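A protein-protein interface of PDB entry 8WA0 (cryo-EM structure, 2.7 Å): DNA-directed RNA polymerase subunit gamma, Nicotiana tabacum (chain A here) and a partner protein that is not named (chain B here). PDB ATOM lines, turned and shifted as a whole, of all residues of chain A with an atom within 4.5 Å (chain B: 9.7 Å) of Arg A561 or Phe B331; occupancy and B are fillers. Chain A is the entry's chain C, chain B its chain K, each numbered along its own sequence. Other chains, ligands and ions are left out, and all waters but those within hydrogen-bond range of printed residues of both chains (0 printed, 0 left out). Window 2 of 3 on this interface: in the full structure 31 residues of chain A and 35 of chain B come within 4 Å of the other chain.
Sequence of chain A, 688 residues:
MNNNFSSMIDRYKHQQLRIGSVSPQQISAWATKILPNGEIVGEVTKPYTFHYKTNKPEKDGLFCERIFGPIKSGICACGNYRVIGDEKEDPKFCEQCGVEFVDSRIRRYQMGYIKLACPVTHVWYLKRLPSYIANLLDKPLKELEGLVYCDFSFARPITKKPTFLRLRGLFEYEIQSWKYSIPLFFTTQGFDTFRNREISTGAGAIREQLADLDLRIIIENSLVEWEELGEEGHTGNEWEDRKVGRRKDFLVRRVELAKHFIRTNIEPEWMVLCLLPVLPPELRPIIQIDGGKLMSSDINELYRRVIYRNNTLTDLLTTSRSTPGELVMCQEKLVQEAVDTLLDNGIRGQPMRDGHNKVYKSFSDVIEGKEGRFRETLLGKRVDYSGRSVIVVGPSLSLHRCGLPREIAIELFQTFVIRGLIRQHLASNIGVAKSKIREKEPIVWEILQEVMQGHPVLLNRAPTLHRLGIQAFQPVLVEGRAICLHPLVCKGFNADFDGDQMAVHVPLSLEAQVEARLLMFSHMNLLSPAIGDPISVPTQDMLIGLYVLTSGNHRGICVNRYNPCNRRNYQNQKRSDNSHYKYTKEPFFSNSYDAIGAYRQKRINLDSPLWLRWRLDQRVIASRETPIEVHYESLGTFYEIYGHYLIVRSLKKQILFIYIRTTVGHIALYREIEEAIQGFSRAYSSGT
The guanidinium group of Arg A561 lies within salt-bridge range of the chain-end carboxylate of Phe B331.
The indole nitrogen (NE1) of Trp B308 is in hydrogen-bond range of the backbone carbonyl oxygen (O) of Asn A560, 3.2 Å away.
The side-chain hydroxyl (OG) of Ser B311 is in hydrogen-bond range of the backbone carbonyl oxygen (O) of Trp B308 (2.9 Å).
Among the printed residues, merely in contact across the chains: Arg A561 with Trp B308 (3.7 Å), Tyr A562 with Trp B308 (3.8 Å) and Asn A563 with Trp B308 (3.7 Å).
Of the printed residues of chain B, Asn A560 touches Trp B308.
Arg A561 touches just these residues of chain B: Trp B308 and Phe B331.
Tyr A562 touches just one residue of chain B: Trp B308.
Printed residues of chain B within 4 Å of Asn A563: Trp B308 (3.7 Å).
Printed residues of chain A within 4 Å of Trp B308: Asn A560 (3.2 Å), Arg A561 (3.7 Å), Tyr A562 (3.8 Å) and Asn A563 (3.7 Å).
Arg B312 touches none of the printed residues of chain A.
Phe B331 touches just one residue of chain A: Arg A561.
The nearest residue of chain B that does not touch Arg A561 is Trp B330 (4.4 Å).
Of the 5 printed residues of chain A, 4 touch a printed residue of chain B.
Of the 9 printed residues of chain B, 2 touch a printed residue of chain A.
Printed residues of chain B that touch a printed residue of chain A: Trp B308 and Phe B331.
Hydrophobic or aromatic side chains of chain B that line the printed part of chain A: Trp B308.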
ATOM      1  N   VAL A 559       6.131  23.521 -12.253  1.00  0.00           N
ATOM      2  CA  VAL A 559       4.724  23.933 -12.167  1.00  0.00           C
ATOM      3  C   VAL A 559       3.736  22.796 -11.840  1.00  0.00           C
ATOM      4  O   VAL A 559       2.722  23.036 -11.183  1.00  0.00           O
ATOM      5  CB  VAL A 559       4.302  24.726 -13.429  1.00  0.00           C
ATOM      6  CG1 VAL A 559       4.262  23.836 -14.659  1.00  0.00           C
ATOM      7  CG2 VAL A 559       2.978  25.443 -13.223  1.00  0.00           C
ATOM      8  N   ASN A 560       4.017  21.567 -12.267  1.00  0.00           N
ATOM      9  CA  ASN A 560       3.164  20.445 -11.992  1.00  0.00           C
ATOM     10  C   ASN A 560       3.912  19.347 -11.268  1.00  0.00           C
ATOM     11  O   ASN A 560       4.983  18.994 -11.694  1.00  0.00           O
ATOM     12  CB  ASN A 560       2.617  19.870 -13.293  1.00  0.00           C
ATOM     13  CG  ASN A 560       1.934  20.880 -14.162  1.00  0.00           C
ATOM     14  OD1 ASN A 560       1.073  21.625 -13.714  1.00  0.00           O
ATOM     15  ND2 ASN A 560       2.290  20.886 -15.433  1.00  0.00           N
ATOM     16  N   ARG A 561       3.402  18.810 -10.172  1.00  0.00           N
ATOM     17  CA  ARG A 561       4.024  17.696  -9.483  1.00  0.00           C
ATOM     18  C   ARG A 561       4.072  16.404 -10.197  1.00  0.00           C
ATOM     19  O   ARG A 561       5.079  15.729 -10.154  1.00  0.00           O
ATOM     20  CB  ARG A 561       3.357  17.452  -8.152  1.00  0.00           C
ATOM     21  CG  ARG A 561       4.174  16.596  -7.213  1.00  0.00           C
ATOM     22  CD  ARG A 561       3.454  16.260  -5.927  1.00  0.00           C
ATOM     23  NE  ARG A 561       4.229  15.300  -5.155  1.00  0.00           N
ATOM     24  CZ  ARG A 561       3.900  14.861  -3.949  1.00  0.00           C
ATOM     25  NH1 ARG A 561       4.672  13.989  -3.327  1.00  0.00           N
ATOM     26  NH2 ARG A 561       2.798  15.298  -3.363  1.00  0.00           N
ATOM     27  N   TYR A 562       3.015  16.033 -10.874  1.00  0.00           N
ATOM     28  CA  TYR A 562       2.925  14.741 -11.493  1.00  0.00           C
ATOM     29  C   TYR A 562       2.759  14.937 -12.964  1.00  0.00           C
ATOM     30  O   TYR A 562       2.364  15.997 -13.368  1.00  0.00           O
ATOM     31  CB  TYR A 562       1.766  13.985 -10.905  1.00  0.00           C
ATOM     32  CG  TYR A 562       1.837  13.609  -9.464  1.00  0.00           C
ATOM     33  CD1 TYR A 562       2.854  12.820  -8.982  1.00  0.00           C
ATOM     34  CD2 TYR A 562       0.846  13.996  -8.593  1.00  0.00           C
ATOM     35  CE1 TYR A 562       2.904  12.461  -7.656  1.00  0.00           C
ATOM     36  CE2 TYR A 562       0.886  13.642  -7.267  1.00  0.00           C
ATOM     37  CZ  TYR A 562       1.916  12.872  -6.808  1.00  0.00           C
ATOM     38  OH  TYR A 562       1.956  12.517  -5.485  1.00  0.00           O
ATOM     39  N   ASN A 563       3.057  13.952 -13.781  1.00  0.00           N
ATOM     40  CA  ASN A 563       3.072  14.112 -15.221  1.00  0.00           C
ATOM     41  C   ASN A 563       1.768  14.534 -15.670  1.00  0.00           C
ATOM     42  O   ASN A 563       0.756  14.011 -15.241  1.00  0.00           O
ATOM     43  CB  ASN A 563       3.431  12.790 -15.890  1.00  0.00           C
ATOM     44  CG  ASN A 563       4.089  12.938 -17.243  1.00  0.00           C
ATOM     45  OD1 ASN A 563       3.702  13.752 -18.067  1.00  0.00           O
ATOM     46  ND2 ASN A 563       5.073  12.098 -17.493  1.00  0.00           N
ATOM     47  N   TRP B 308       7.283  18.883 -19.365  1.00  0.00           N
ATOM     48  CA  TRP B 308       7.565  17.996 -18.276  1.00  0.00           C
ATOM     49  C   TRP B 308       8.568  16.937 -18.598  1.00  0.00           C
ATOM     50  O   TRP B 308       9.440  16.672 -17.784  1.00  0.00           O
ATOM     51  CB  TRP B 308       6.314  17.335 -17.759  1.00  0.00           C
ATOM     52  CG  TRP B 308       6.269  17.018 -16.305  1.00  0.00           C
ATOM     53  CD1 TRP B 308       5.756  17.795 -15.325  1.00  0.00           C
ATOM     54  CD2 TRP B 308       6.715  15.821 -15.671  1.00  0.00           C
ATOM     55  NE1 TRP B 308       5.868  17.174 -14.120  1.00  0.00           N
ATOM     56  CE2 TRP B 308       6.461  15.958 -14.304  1.00  0.00           C
ATOM     57  CE3 TRP B 308       7.318  14.653 -16.125  1.00  0.00           C
ATOM     58  CZ2 TRP B 308       6.786  14.979 -13.393  1.00  0.00           C
ATOM     59  CZ3 TRP B 308       7.638  13.691 -15.224  1.00  0.00           C
ATOM     60  CH2 TRP B 308       7.373  13.852 -13.872  1.00  0.00           C
ATOM     61  N   SER B 311      12.156  18.747 -18.941  1.00  0.00           N
ATOM     62  CA  SER B 311      12.598  19.233 -17.677  1.00  0.00           C
ATOM     63  C   SER B 311      13.023  18.121 -16.758  1.00  0.00           C
ATOM     64  O   SER B 311      13.997  18.277 -16.051  1.00  0.00           O
ATOM     65  CB  SER B 311      11.494  20.037 -17.068  1.00  0.00           C
ATOM     66  OG  SER B 311      10.322  19.277 -16.916  1.00  0.00           O
ATOM     67  N   ARG B 312      12.322  16.997 -16.734  1.00  0.00           N
ATOM     68  CA  ARG B 312      12.739  15.903 -15.914  1.00  0.00           C
ATOM     69  C   ARG B 312      14.039  15.303 -16.292  1.00  0.00           C
ATOM     70  O   ARG B 312      14.893  15.113 -15.442  1.00  0.00           O
ATOM     71  CB  ARG B 312      11.694  14.831 -15.782  1.00  0.00           C
ATOM     72  CG  ARG B 312      11.336  14.496 -14.363  1.00  0.00           C
ATOM     73  CD  ARG B 312      11.333  13.007 -14.138  1.00  0.00           C
ATOM     74  NE  ARG B 312      12.612  12.543 -13.648  1.00  0.00           N
ATOM     75  CZ  ARG B 312      12.761  11.454 -12.920  1.00  0.00           C
ATOM     76  NH1 ARG B 312      11.706  10.736 -12.595  1.00  0.00           N
ATOM     77  NH2 ARG B 312      13.956  11.085 -12.509  1.00  0.00           N
ATOM     78  N   MET B 315      17.008  17.744 -15.172  1.00  0.00           N
ATOM     79  CA  MET B 315      17.355  17.734 -13.771  1.00  0.00           C
ATOM     80  C   MET B 315      18.145  16.528 -13.370  1.00  0.00           C
ATOM     81  O   MET B 315      19.061  16.641 -12.574  1.00  0.00           O
ATOM     82  CB  MET B 315      16.155  17.872 -12.885  1.00  0.00           C
ATOM     83  CG  MET B 315      16.430  18.150 -11.425  1.00  0.00           C
ATOM     84  SD  MET B 315      16.778  19.882 -11.122  1.00  0.00           S
ATOM     85  CE  MET B 315      17.111  19.876  -9.365  1.00  0.00           C
ATOM     86  N   LEU B 319      21.868  16.333 -11.557  1.00  0.00           N
ATOM     87  CA  LEU B 319      22.064  15.762 -10.277  1.00  0.00           C
ATOM     88  C   LEU B 319      22.901  14.517 -10.247  1.00  0.00           C
ATOM     89  O   LEU B 319      23.305  14.088  -9.186  1.00  0.00           O
ATOM     90  CB  LEU B 319      20.723  15.587  -9.577  1.00  0.00           C
ATOM     91  CG  LEU B 319      19.789  16.729  -9.239  1.00  0.00           C
ATOM     92  CD1 LEU B 319      18.547  16.104  -8.654  1.00  0.00           C
ATOM     93  CD2 LEU B 319      20.428  17.658  -8.236  1.00  0.00           C
ATOM     94  N   SER B 328      19.703   8.318  -3.377  1.00  0.00           N
ATOM     95  CA  SER B 328      18.639   9.312  -3.282  1.00  0.00           C
ATOM     96  C   SER B 328      17.298   8.934  -3.913  1.00  0.00           C
ATOM     97  O   SER B 328      17.235   7.952  -4.615  1.00  0.00           O
ATOM     98  CB  SER B 328      19.156  10.576  -3.897  1.00  0.00           C
ATOM     99  OG  SER B 328      20.419  10.903  -3.399  1.00  0.00           O
ATOM    100  N   ASN B 329      16.226   9.690  -3.676  1.00  0.00           N
ATOM    101  CA  ASN B 329      14.900   9.397  -4.186  1.00  0.00           C
ATOM    102  C   ASN B 329      14.266  10.599  -4.859  1.00  0.00           C
ATOM    103  O   ASN B 329      14.325  11.675  -4.298  1.00  0.00           O
ATOM    104  CB  ASN B 329      14.073   8.977  -2.968  1.00  0.00           C
ATOM    105  CG  ASN B 329      12.865   8.166  -3.277  1.00  0.00           C
ATOM    106  OD1 ASN B 329      11.850   8.687  -3.724  1.00  0.00           O
ATOM    107  ND2 ASN B 329      12.928   6.888  -2.956  1.00  0.00           N
ATOM    108  N   TRP B 330      13.675  10.473  -6.045  1.00  0.00           N
ATOM    109  CA  TRP B 330      12.924  11.569  -6.647  1.00  0.00           C
ATOM    110  C   TRP B 330      11.657  11.735  -5.892  1.00  0.00           C
ATOM    111  O   TRP B 330      11.023  10.761  -5.563  1.00  0.00           O
ATOM    112  CB  TRP B 330      12.510  11.288  -8.056  1.00  0.00           C
ATOM    113  CG  TRP B 330      12.383  12.517  -8.893  1.00  0.00           C
ATOM    114  CD1 TRP B 330      13.394  13.332  -9.308  1.00  0.00           C
ATOM    115  CD2 TRP B 330      11.184  13.073  -9.423  1.00  0.00           C
ATOM    116  NE1 TRP B 330      12.896  14.366 -10.060  1.00  0.00           N
ATOM    117  CE2 TRP B 330      11.540  14.228 -10.144  1.00  0.00           C
ATOM    118  CE3 TRP B 330       9.849  12.713  -9.355  1.00  0.00           C
ATOM    119  CZ2 TRP B 330      10.613  15.016 -10.782  1.00  0.00           C
ATOM    120  CZ3 TRP B 330       8.932  13.498  -9.991  1.00  0.00           C
ATOM    121  CH2 TRP B 330       9.312  14.634 -10.700  1.00  0.00           C
ATOM    122  N   PHE B 331      11.230  12.951  -5.644  1.00  0.00           N
ATOM    123  CA  PHE B 331      10.060  13.160  -4.851  1.00  0.00           C
ATOM    124  C   PHE B 331       9.159  14.220  -5.395  1.00  0.00           C
ATOM    125  O   PHE B 331       8.003  14.327  -4.999  1.00  0.00           O
ATOM    126  CB  PHE B 331      10.397  13.400  -3.384  1.00  0.00           C
ATOM    127  CG  PHE B 331      11.320  14.538  -3.116  1.00  0.00           C
ATOM    128  CD1 PHE B 331      10.865  15.836  -3.109  1.00  0.00           C
ATOM    129  CD2 PHE B 331      12.627  14.296  -2.779  1.00  0.00           C
ATOM    130  CE1 PHE B 331      11.709  16.878  -2.837  1.00  0.00           C
ATOM    131  CE2 PHE B 331      13.481  15.328  -2.509  1.00  0.00           C
ATOM    132  CZ  PHE B 331      13.022  16.622  -2.534  1.00  0.00           C
ATOM    133  OXT PHE B 331       9.525  14.998  -6.220  1.00  0.00           O
